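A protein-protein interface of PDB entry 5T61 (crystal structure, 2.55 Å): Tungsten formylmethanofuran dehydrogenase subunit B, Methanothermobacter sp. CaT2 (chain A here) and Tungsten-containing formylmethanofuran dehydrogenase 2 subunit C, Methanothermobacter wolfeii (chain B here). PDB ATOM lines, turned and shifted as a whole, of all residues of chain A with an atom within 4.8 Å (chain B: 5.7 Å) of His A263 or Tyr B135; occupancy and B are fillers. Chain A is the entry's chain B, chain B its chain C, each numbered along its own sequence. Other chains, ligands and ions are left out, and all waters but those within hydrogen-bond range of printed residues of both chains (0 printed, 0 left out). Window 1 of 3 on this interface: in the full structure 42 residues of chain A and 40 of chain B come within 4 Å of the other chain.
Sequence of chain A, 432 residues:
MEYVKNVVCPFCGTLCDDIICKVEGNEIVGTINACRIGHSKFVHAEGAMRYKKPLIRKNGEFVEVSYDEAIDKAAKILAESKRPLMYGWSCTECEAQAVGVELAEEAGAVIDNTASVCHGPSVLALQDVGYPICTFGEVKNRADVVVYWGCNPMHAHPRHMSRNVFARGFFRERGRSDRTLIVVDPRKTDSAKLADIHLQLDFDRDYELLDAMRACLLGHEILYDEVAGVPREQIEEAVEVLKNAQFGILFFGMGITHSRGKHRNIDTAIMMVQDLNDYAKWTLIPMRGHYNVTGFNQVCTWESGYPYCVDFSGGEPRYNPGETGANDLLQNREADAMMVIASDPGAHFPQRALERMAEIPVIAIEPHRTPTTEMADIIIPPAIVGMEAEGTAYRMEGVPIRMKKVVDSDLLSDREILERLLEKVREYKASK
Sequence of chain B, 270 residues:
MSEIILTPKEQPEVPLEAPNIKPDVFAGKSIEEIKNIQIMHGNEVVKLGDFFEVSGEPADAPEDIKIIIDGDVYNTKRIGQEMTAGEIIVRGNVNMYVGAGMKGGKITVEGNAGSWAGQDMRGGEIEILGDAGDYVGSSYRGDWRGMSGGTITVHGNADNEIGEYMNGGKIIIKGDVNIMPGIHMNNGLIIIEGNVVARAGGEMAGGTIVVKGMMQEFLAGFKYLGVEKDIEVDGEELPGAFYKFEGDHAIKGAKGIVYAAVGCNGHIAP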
ATOM      1  N   PRO A 121       4.436  15.289 -13.299  1.00  0.00           N
ATOM      2  CA  PRO A 121       4.242  16.725 -13.562  1.00  0.00           C
ATOM      3  C   PRO A 121       3.221  17.382 -12.653  1.00  0.00           C
ATOM      4  O   PRO A 121       3.400  18.546 -12.274  1.00  0.00           O
ATOM      5  CB  PRO A 121       3.784  16.748 -15.026  1.00  0.00           C
ATOM      6  CG  PRO A 121       4.369  15.527 -15.620  1.00  0.00           C
ATOM      7  CD  PRO A 121       4.357  14.491 -14.536  1.00  0.00           C
ATOM      8  N   LEU A 124       5.203  17.960  -9.434  1.00  0.00           N
ATOM      9  CA  LEU A 124       5.999  19.183  -9.542  1.00  0.00           C
ATOM     10  C   LEU A 124       5.123  20.426  -9.433  1.00  0.00           C
ATOM     11  O   LEU A 124       5.471  21.380  -8.727  1.00  0.00           O
ATOM     12  CB  LEU A 124       6.787  19.209 -10.856  1.00  0.00           C
ATOM     13  CG  LEU A 124       7.874  18.165 -11.137  1.00  0.00           C
ATOM     14  CD1 LEU A 124       8.401  18.304 -12.563  1.00  0.00           C
ATOM     15  CD2 LEU A 124       9.008  18.270 -10.134  1.00  0.00           C
ATOM     16  N   ALA A 125       3.977  20.430 -10.114  1.00  0.00           N
ATOM     17  CA  ALA A 125       3.107  21.600 -10.094  1.00  0.00           C
ATOM     18  C   ALA A 125       2.545  21.858  -8.702  1.00  0.00           C
ATOM     19  O   ALA A 125       2.535  23.002  -8.233  1.00  0.00           O
ATOM     20  CB  ALA A 125       1.972  21.429 -11.100  1.00  0.00           C
ATOM     21  N   GLY A 261       4.538  21.836 -22.010  1.00  0.00           N
ATOM     22  CA  GLY A 261       4.411  22.526 -20.763  1.00  0.00           C
ATOM     23  C   GLY A 261       4.383  21.576 -19.588  1.00  0.00           C
ATOM     24  O   GLY A 261       4.864  21.925 -18.504  1.00  0.00           O
ATOM     25  N   LYS A 262       3.840  20.373 -19.796  1.00  0.00           N
ATOM     26  CA  LYS A 262       3.832  19.298 -18.812  1.00  0.00           C
ATOM     27  C   LYS A 262       3.389  19.808 -17.447  1.00  0.00           C
ATOM     28  O   LYS A 262       2.202  20.090 -17.252  1.00  0.00           O
ATOM     29  CB  LYS A 262       5.207  18.621 -18.774  1.00  0.00           C
ATOM     30  CG  LYS A 262       5.480  17.863 -20.076  1.00  0.00           C
ATOM     31  CD  LYS A 262       6.888  17.320 -20.223  1.00  0.00           C
ATOM     32  CE  LYS A 262       7.002  16.551 -21.542  1.00  0.00           C
ATOM     33  NZ  LYS A 262       8.403  16.260 -21.957  1.00  0.00           N
ATOM     34  N   HIS A 263       4.318  19.924 -16.494  1.00  0.00           N
ATOM     35  CA  HIS A 263       3.924  20.305 -15.141  1.00  0.00           C
ATOM     36  C   HIS A 263       3.343  21.713 -15.092  1.00  0.00           C
ATOM     37  O   HIS A 263       2.536  22.018 -14.207  1.00  0.00           O
ATOM     38  CB  HIS A 263       5.105  20.192 -14.177  1.00  0.00           C
ATOM     39  CG  HIS A 263       6.249  21.092 -14.508  1.00  0.00           C
ATOM     40  ND1 HIS A 263       6.958  20.993 -15.685  1.00  0.00           N
ATOM     41  CD2 HIS A 263       6.802  22.116 -13.817  1.00  0.00           C
ATOM     42  CE1 HIS A 263       7.905  21.913 -15.700  1.00  0.00           C
ATOM     43  NE2 HIS A 263       7.831  22.609 -14.580  1.00  0.00           N
ATOM     44  N   ARG A 264       3.733  22.586 -16.019  1.00  0.00           N
ATOM     45  CA  ARG A 264       3.196  23.937 -15.984  1.00  0.00           C
ATOM     46  C   ARG A 264       1.774  24.015 -16.520  1.00  0.00           C
ATOM     47  O   ARG A 264       1.068  24.984 -16.216  1.00  0.00           O
ATOM     48  CB  ARG A 264       4.099  24.899 -16.758  1.00  0.00           C
ATOM     49  CG  ARG A 264       5.516  25.002 -16.208  1.00  0.00           C
ATOM     50  CD  ARG A 264       5.523  25.536 -14.787  1.00  0.00           C
ATOM     51  NE  ARG A 264       6.869  25.558 -14.224  1.00  0.00           N
ATOM     52  CZ  ARG A 264       7.134  25.556 -12.923  1.00  0.00           C
ATOM     53  NH1 ARG A 264       6.147  25.524 -12.041  1.00  0.00           N
ATOM     54  NH2 ARG A 264       8.390  25.587 -12.504  1.00  0.00           N
ATOM     55  N   ASN A 265       1.326  23.025 -17.300  1.00  0.00           N
ATOM     56  CA  ASN A 265      -0.098  22.953 -17.612  1.00  0.00           C
ATOM     57  C   ASN A 265      -0.907  22.657 -16.355  1.00  0.00           C
ATOM     58  O   ASN A 265      -1.979  23.238 -16.147  1.00  0.00           O
ATOM     59  CB  ASN A 265      -0.378  21.896 -18.685  1.00  0.00           C
ATOM     60  CG  ASN A 265       0.316  22.190 -20.010  1.00  0.00           C
ATOM     61  OD1 ASN A 265       0.553  23.344 -20.369  1.00  0.00           O
ATOM     62  ND2 ASN A 265       0.595  21.134 -20.767  1.00  0.00           N
ATOM     63  N   ILE A 266      -0.406  21.760 -15.503  1.00  0.00           N
ATOM     64  CA  ILE A 266      -1.089  21.465 -14.247  1.00  0.00           C
ATOM     65  C   ILE A 266      -1.033  22.675 -13.330  1.00  0.00           C
ATOM     66  O   ILE A 266      -1.996  22.982 -12.616  1.00  0.00           O
ATOM     67  CB  ILE A 266      -0.463  20.236 -13.564  1.00  0.00           C
ATOM     68  CG1 ILE A 266      -0.114  19.148 -14.579  1.00  0.00           C
ATOM     69  CG2 ILE A 266      -1.398  19.699 -12.489  1.00  0.00           C
ATOM     70  CD1 ILE A 266      -1.265  18.711 -15.421  1.00  0.00           C
ATOM     71  N   ASP A 267       0.112  23.361 -13.325  1.00  0.00           N
ATOM     72  CA  ASP A 267       0.322  24.543 -12.500  1.00  0.00           C
ATOM     73  C   ASP A 267      -0.786  25.563 -12.718  1.00  0.00           C
ATOM     74  O   ASP A 267      -1.459  25.983 -11.771  1.00  0.00           O
ATOM     75  CB  ASP A 267       1.706  25.129 -12.823  1.00  0.00           C
ATOM     76  CG  ASP A 267       1.989  26.465 -12.135  1.00  0.00           C
ATOM     77  OD1 ASP A 267       1.118  27.354 -12.080  1.00  0.00           O
ATOM     78  OD2 ASP A 267       3.126  26.628 -11.645  1.00  0.00           O
ATOM     79  N   SER B 115      21.441  21.259 -17.384  1.00  0.00           N
ATOM     80  CA  SER B 115      20.331  21.952 -16.751  1.00  0.00           C
ATOM     81  C   SER B 115      20.760  22.549 -15.414  1.00  0.00           C
ATOM     82  O   SER B 115      21.740  22.125 -14.798  1.00  0.00           O
ATOM     83  CB  SER B 115      19.159  20.997 -16.542  1.00  0.00           C
ATOM     84  OG  SER B 115      18.584  20.613 -17.774  1.00  0.00           O
ATOM     85  N   TRP B 116      20.011  23.566 -14.980  1.00  0.00           N
ATOM     86  CA  TRP B 116      20.185  24.204 -13.673  1.00  0.00           C
ATOM     87  C   TRP B 116      21.526  24.923 -13.554  1.00  0.00           C
ATOM     88  O   TRP B 116      22.092  25.017 -12.461  1.00  0.00           O
ATOM     89  CB  TRP B 116      20.001  23.196 -12.529  1.00  0.00           C
ATOM     90  CG  TRP B 116      18.589  22.696 -12.443  1.00  0.00           C
ATOM     91  CD1 TRP B 116      17.494  23.403 -12.038  1.00  0.00           C
ATOM     92  CD2 TRP B 116      18.112  21.394 -12.810  1.00  0.00           C
ATOM     93  NE1 TRP B 116      16.369  22.619 -12.116  1.00  0.00           N
ATOM     94  CE2 TRP B 116      16.721  21.382 -12.587  1.00  0.00           C
ATOM     95  CE3 TRP B 116      18.728  20.235 -13.294  1.00  0.00           C
ATOM     96  CZ2 TRP B 116      15.935  20.257 -12.835  1.00  0.00           C
ATOM     97  CZ3 TRP B 116      17.945  19.121 -13.543  1.00  0.00           C
ATOM     98  CH2 TRP B 116      16.565  19.141 -13.312  1.00  0.00           C
ATOM     99  N   ALA B 117      22.044  25.430 -14.669  1.00  0.00           N
ATOM    100  CA  ALA B 117      23.202  26.312 -14.619  1.00  0.00           C
ATOM    101  C   ALA B 117      22.852  27.596 -13.879  1.00  0.00           C
ATOM    102  O   ALA B 117      21.982  28.355 -14.314  1.00  0.00           O
ATOM    103  CB  ALA B 117      23.683  26.625 -16.034  1.00  0.00           C
ATOM    104  N   GLY B 118      23.531  27.837 -12.763  1.00  0.00           N
ATOM    105  CA  GLY B 118      23.271  29.033 -11.989  1.00  0.00           C
ATOM    106  C   GLY B 118      21.971  29.031 -11.217  1.00  0.00           C
ATOM    107  O   GLY B 118      21.479  30.101 -10.855  1.00  0.00           O
ATOM    108  N   GLN B 119      21.392  27.857 -10.972  1.00  0.00           N
ATOM    109  CA  GLN B 119      20.214  27.751 -10.120  1.00  0.00           C
ATOM    110  C   GLN B 119      20.484  28.361  -8.748  1.00  0.00           C
ATOM    111  O   GLN B 119      21.534  28.124  -8.147  1.00  0.00           O
ATOM    112  CB  GLN B 119      19.804  26.283  -9.987  1.00  0.00           C
ATOM    113  CG  GLN B 119      18.961  25.960  -8.763  1.00  0.00           C
ATOM    114  CD  GLN B 119      18.733  24.479  -8.604  1.00  0.00           C
ATOM    115  OE1 GLN B 119      17.595  24.017  -8.546  1.00  0.00           O
ATOM    116  NE2 GLN B 119      19.808  23.707  -8.545  1.00  0.00           N
ATOM    117  N   GLY B 133      21.136  24.071 -20.947  1.00  0.00           N
ATOM    118  CA  GLY B 133      19.986  23.201 -20.805  1.00  0.00           C
ATOM    119  C   GLY B 133      18.764  23.928 -20.293  1.00  0.00           C
ATOM    120  O   GLY B 133      18.572  25.125 -20.532  1.00  0.00           O
ATOM    121  N   ASP B 134      17.914  23.188 -19.590  1.00  0.00           N
ATOM    122  CA  ASP B 134      16.738  23.770 -18.966  1.00  0.00           C
ATOM    123  C   ASP B 134      17.113  24.473 -17.665  1.00  0.00           C
ATOM    124  O   ASP B 134      18.186  24.255 -17.097  1.00  0.00           O
ATOM    125  CB  ASP B 134      15.690  22.691 -18.685  1.00  0.00           C
ATOM    126  CG  ASP B 134      15.342  21.875 -19.915  1.00  0.00           C
ATOM    127  OD1 ASP B 134      14.614  22.392 -20.785  1.00  0.00           O
ATOM    128  OD2 ASP B 134      15.792  20.716 -20.013  1.00  0.00           O
ATOM    129  N   TYR B 135      16.218  25.351 -17.210  1.00  0.00           N
ATOM    130  CA  TYR B 135      16.273  25.910 -15.856  1.00  0.00           C
ATOM    131  C   TYR B 135      17.546  26.719 -15.601  1.00  0.00           C
ATOM    132  O   TYR B 135      18.115  26.673 -14.508  1.00  0.00           O
ATOM    133  CB  TYR B 135      16.131  24.807 -14.801  1.00  0.00           C
ATOM    134  CG  TYR B 135      14.784  24.116 -14.754  1.00  0.00           C
ATOM    135  CD1 TYR B 135      13.656  24.773 -14.277  1.00  0.00           C
ATOM    136  CD2 TYR B 135      14.644  22.802 -15.180  1.00  0.00           C
ATOM    137  CE1 TYR B 135      12.427  24.139 -14.228  1.00  0.00           C
ATOM    138  CE2 TYR B 135      13.422  22.162 -15.138  1.00  0.00           C
ATOM    139  CZ  TYR B 135      12.318  22.832 -14.661  1.00  0.00           C
ATOM    140  OH  TYR B 135      11.102  22.188 -14.621  1.00  0.00           O
ATOM    141  N   VAL B 136      18.006  27.469 -16.606  1.00  0.00           N
ATOM    142  CA  VAL B 136      19.090  28.415 -16.360  1.00  0.00           C
ATOM    143  C   VAL B 136      18.617  29.452 -15.356  1.00  0.00           C
ATOM    144  O   VAL B 136      17.587  30.106 -15.555  1.00  0.00           O
ATOM    145  CB  VAL B 136      19.556  29.074 -17.665  1.00  0.00           C
ATOM    146  CG1 VAL B 136      20.614  30.127 -17.381  1.00  0.00           C
ATOM    147  CG2 VAL B 136      20.077  28.031 -18.639  1.00  0.00           C
ATOM    148  N   GLY B 137      19.371  29.612 -14.274  1.00  0.00           N
ATOM    149  CA  GLY B 137      18.997  30.584 -13.258  1.00  0.00           C
ATOM    150  C   GLY B 137      17.631  30.329 -12.657  1.00  0.00           C
ATOM    151  O   GLY B 137      16.866  31.274 -12.430  1.00  0.00           O
ATOM    152  N   SER B 138      17.300  29.065 -12.411  1.00  0.00           N
ATOM    153  CA  SER B 138      15.989  28.696 -11.906  1.00  0.00           C
ATOM    154  C   SER B 138      15.993  28.667 -10.380  1.00  0.00           C
ATOM    155  O   SER B 138      16.994  28.958  -9.721  1.00  0.00           O
ATOM    156  CB  SER B 138      15.567  27.335 -12.450  1.00  0.00           C
ATOM    157  OG  SER B 138      16.272  26.301 -11.782  1.00  0.00           O
ATOM    158  N   SER B 139      14.844  28.323  -9.811  1.00  0.00           N
ATOM    159  CA  SER B 139      14.724  28.024  -8.397  1.00  0.00           C
ATOM    160  C   SER B 139      14.807  26.513  -8.188  1.00  0.00           C
ATOM    161  O   SER B 139      15.018  25.737  -9.125  1.00  0.00           O
ATOM    162  CB  SER B 139      13.419  28.601  -7.841  1.00  0.00           C
ATOM    163  OG  SER B 139      12.296  27.866  -8.292  1.00  0.00           O
ATOM    164  N   ARG B 141      12.791  22.994  -6.653  1.00  0.00           N
ATOM    165  CA  ARG B 141      11.447  22.433  -6.523  1.00  0.00           C
ATOM    166  C   ARG B 141      10.725  22.972  -5.298  1.00  0.00           C
ATOM    167  O   ARG B 141      11.259  22.947  -4.187  1.00  0.00           O
ATOM    168  CB  ARG B 141      11.516  20.908  -6.424  1.00  0.00           C
ATOM    169  CG  ARG B 141      12.178  20.239  -7.589  1.00  0.00           C
ATOM    170  CD  ARG B 141      11.589  20.745  -8.873  1.00  0.00           C
ATOM    171  NE  ARG B 141      12.118  20.036 -10.027  1.00  0.00           N
ATOM    172  CZ  ARG B 141      11.833  20.359 -11.283  1.00  0.00           C
ATOM    173  NH1 ARG B 141      11.036  21.387 -11.533  1.00  0.00           N
ATOM    174  NH2 ARG B 141      12.346  19.659 -12.285  1.00  0.00           N
ATOM    175  N   ASN B 160      14.158  25.144 -21.807  1.00  0.00           N
ATOM    176  CA  ASN B 160      12.929  25.531 -21.122  1.00  0.00           C
ATOM    177  C   ASN B 160      13.167  26.195 -19.771  1.00  0.00           C
ATOM    178  O   ASN B 160      14.151  25.933 -19.076  1.00  0.00           O
ATOM    179  CB  ASN B 160      12.028  24.312 -20.900  1.00  0.00           C
ATOM    180  CG  ASN B 160      11.342  23.856 -22.169  1.00  0.00           C
ATOM    181  OD1 ASN B 160      11.543  24.430 -23.234  1.00  0.00           O
ATOM    182  ND2 ASN B 160      10.488  22.846 -22.051  1.00  0.00           N
ATOM    183  N   GLU B 161      12.222  27.086 -19.424  1.00  0.00           N
ATOM    184  CA  GLU B 161      12.030  27.627 -18.071  1.00  0.00           C
ATOM    185  C   GLU B 161      13.283  28.282 -17.510  1.00  0.00           C
ATOM    186  O   GLU B 161      13.601  28.146 -16.326  1.00  0.00           O
ATOM    187  CB  GLU B 161      11.515  26.554 -17.113  1.00  0.00           C
ATOM    188  CG  GLU B 161      10.179  25.970 -17.503  1.00  0.00           C
ATOM    189  CD  GLU B 161       9.701  24.958 -16.490  1.00  0.00           C
ATOM    190  OE1 GLU B 161       9.293  25.357 -15.375  1.00  0.00           O
ATOM    191  OE2 GLU B 161       9.762  23.754 -16.806  1.00  0.00           O
ATOM    192  N   ILE B 162      13.991  29.020 -18.355  1.00  0.00           N
ATOM    193  CA  ILE B 162      15.106  29.813 -17.868  1.00  0.00           C
ATOM    194  C   ILE B 162      14.568  30.971 -17.031  1.00  0.00           C
ATOM    195  O   ILE B 162      13.546  31.585 -17.369  1.00  0.00           O
ATOM    196  CB  ILE B 162      15.972  30.254 -19.061  1.00  0.00           C
ATOM    197  CG1 ILE B 162      15.128  30.858 -20.187  1.00  0.00           C
ATOM    198  CG2 ILE B 162      16.736  29.071 -19.612  1.00  0.00           C
ATOM    199  CD1 ILE B 162      14.882  32.331 -20.051  1.00  0.00           C
ATOM    200  N   GLY B 163      15.229  31.251 -15.907  1.00  0.00           N
ATOM    201  CA  GLY B 163      14.763  32.280 -14.996  1.00  0.00           C
ATOM    202  C   GLY B 163      13.499  31.934 -14.238  1.00  0.00           C
ATOM    203  O   GLY B 163      12.800  32.838 -13.773  1.00  0.00           O
ATOM    204  N   GLU B 164      13.177  30.645 -14.120  1.00  0.00           N
ATOM    205  CA  GLU B 164      12.030  30.196 -13.338  1.00  0.00           C
ATOM    206  C   GLU B 164      12.060  30.794 -11.940  1.00  0.00           C
ATOM    207  O   GLU B 164      13.045  30.642 -11.211  1.00  0.00           O
ATOM    208  CB  GLU B 164      12.020  28.667 -13.260  1.00  0.00           C
ATOM    209  CG  GLU B 164      10.817  28.074 -12.532  1.00  0.00           C
ATOM    210  CD  GLU B 164      11.210  27.258 -11.313  1.00  0.00           C
ATOM    211  OE1 GLU B 164      12.368  27.385 -10.859  1.00  0.00           O
ATOM    212  OE2 GLU B 164      10.362  26.488 -10.812  1.00  0.00           O
ATOM    213  N   MET B 180       8.457  28.868 -22.179  1.00  0.00           N
ATOM    214  CA  MET B 180       8.260  29.335 -20.818  1.00  0.00           C
ATOM    215  C   MET B 180       9.490  30.044 -20.257  1.00  0.00           C
ATOM    216  O   MET B 180       9.829  29.820 -19.089  1.00  0.00           O
ATOM    217  CB  MET B 180       7.821  28.168 -19.933  1.00  0.00           C
ATOM    218  CG  MET B 180       6.567  27.525 -20.487  1.00  0.00           C
ATOM    219  SD  MET B 180       5.770  26.322 -19.434  1.00  0.00           S
ATOM    220  CE  MET B 180       6.920  24.957 -19.546  1.00  0.00           C
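OE2 of Glu B161 sits at hydrogen-bond distance from OH of Tyr B135, 3.0 Å away. OG of Ser B139 lies within hydrogen-bond range of OE1 of Glu B164, 2.6 Å away. The guanidinium group (NE) of Arg A264 is in hydrogen-bond range of a ring nitrogen (NE2) of His A263, 3.1 Å away. The backbone NH of Tyr B135 lies within hydrogen-bond range of the backbone carbonyl oxygen of Asn B160. The side-chain hydroxyl of Ser B138 sits at hydrogen-bond distance from the backbone carbonyl oxygen of Tyr B135 (3.3 Å). NH1 of Arg A264 lies within salt-bridge range of OD2 of Asp A267, at 3.2 Å.
Printed residues of chain B within 4 Å of Gly A261: Met B180 (3.7 Å). Of chain B, only Tyr B135 (3.3 Å) and Glu B161 (2.8 Å) come within 4 Å of His A263. Printed residues of chain B within 4 Å of Arg A264: Glu B161, Glu B164 and Met B180. Tyr B135 touches just one residue of chain A: His A263. Printed residues of chain A within 4 Å of Arg B141: Leu A124 (3.6 Å). The nearest residue of chain A that does not touch Tyr B135 is Arg A264 (4.6 Å).
Of the 10 printed residues of chain A, 4 touch a printed residue of chain B. Among the printed residues, 7 pairs touch across the chains. Among the printed residues, Asp or Glu carboxylates within 4 Å of a Lys or Arg side-chain nitrogen of the other chain: Arg A264 with Glu B161 (2.7 Å) and Arg A264 with Glu B164 (2.8 Å).
Among the printed residues, merely in contact across the chains: Leu A124 with Arg B141, Gly A261 with Met B180 and Arg A264 with Met B180.
NE2 of His A263 lies within hydrogen-bond range of OH of Tyr B135 (3.3 Å). OE1 of Glu B161 lies within salt-bridge range of NE of Arg A264 (2.7 Å). The side-chain carboxylate of Glu B164 lies within salt-bridge range of the guanidinium group of Arg A264 (2.8 Å). A ring nitrogen (NE2) of His A263 sits close to the side-chain carboxylate of Glu B161 (3.2 Å).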
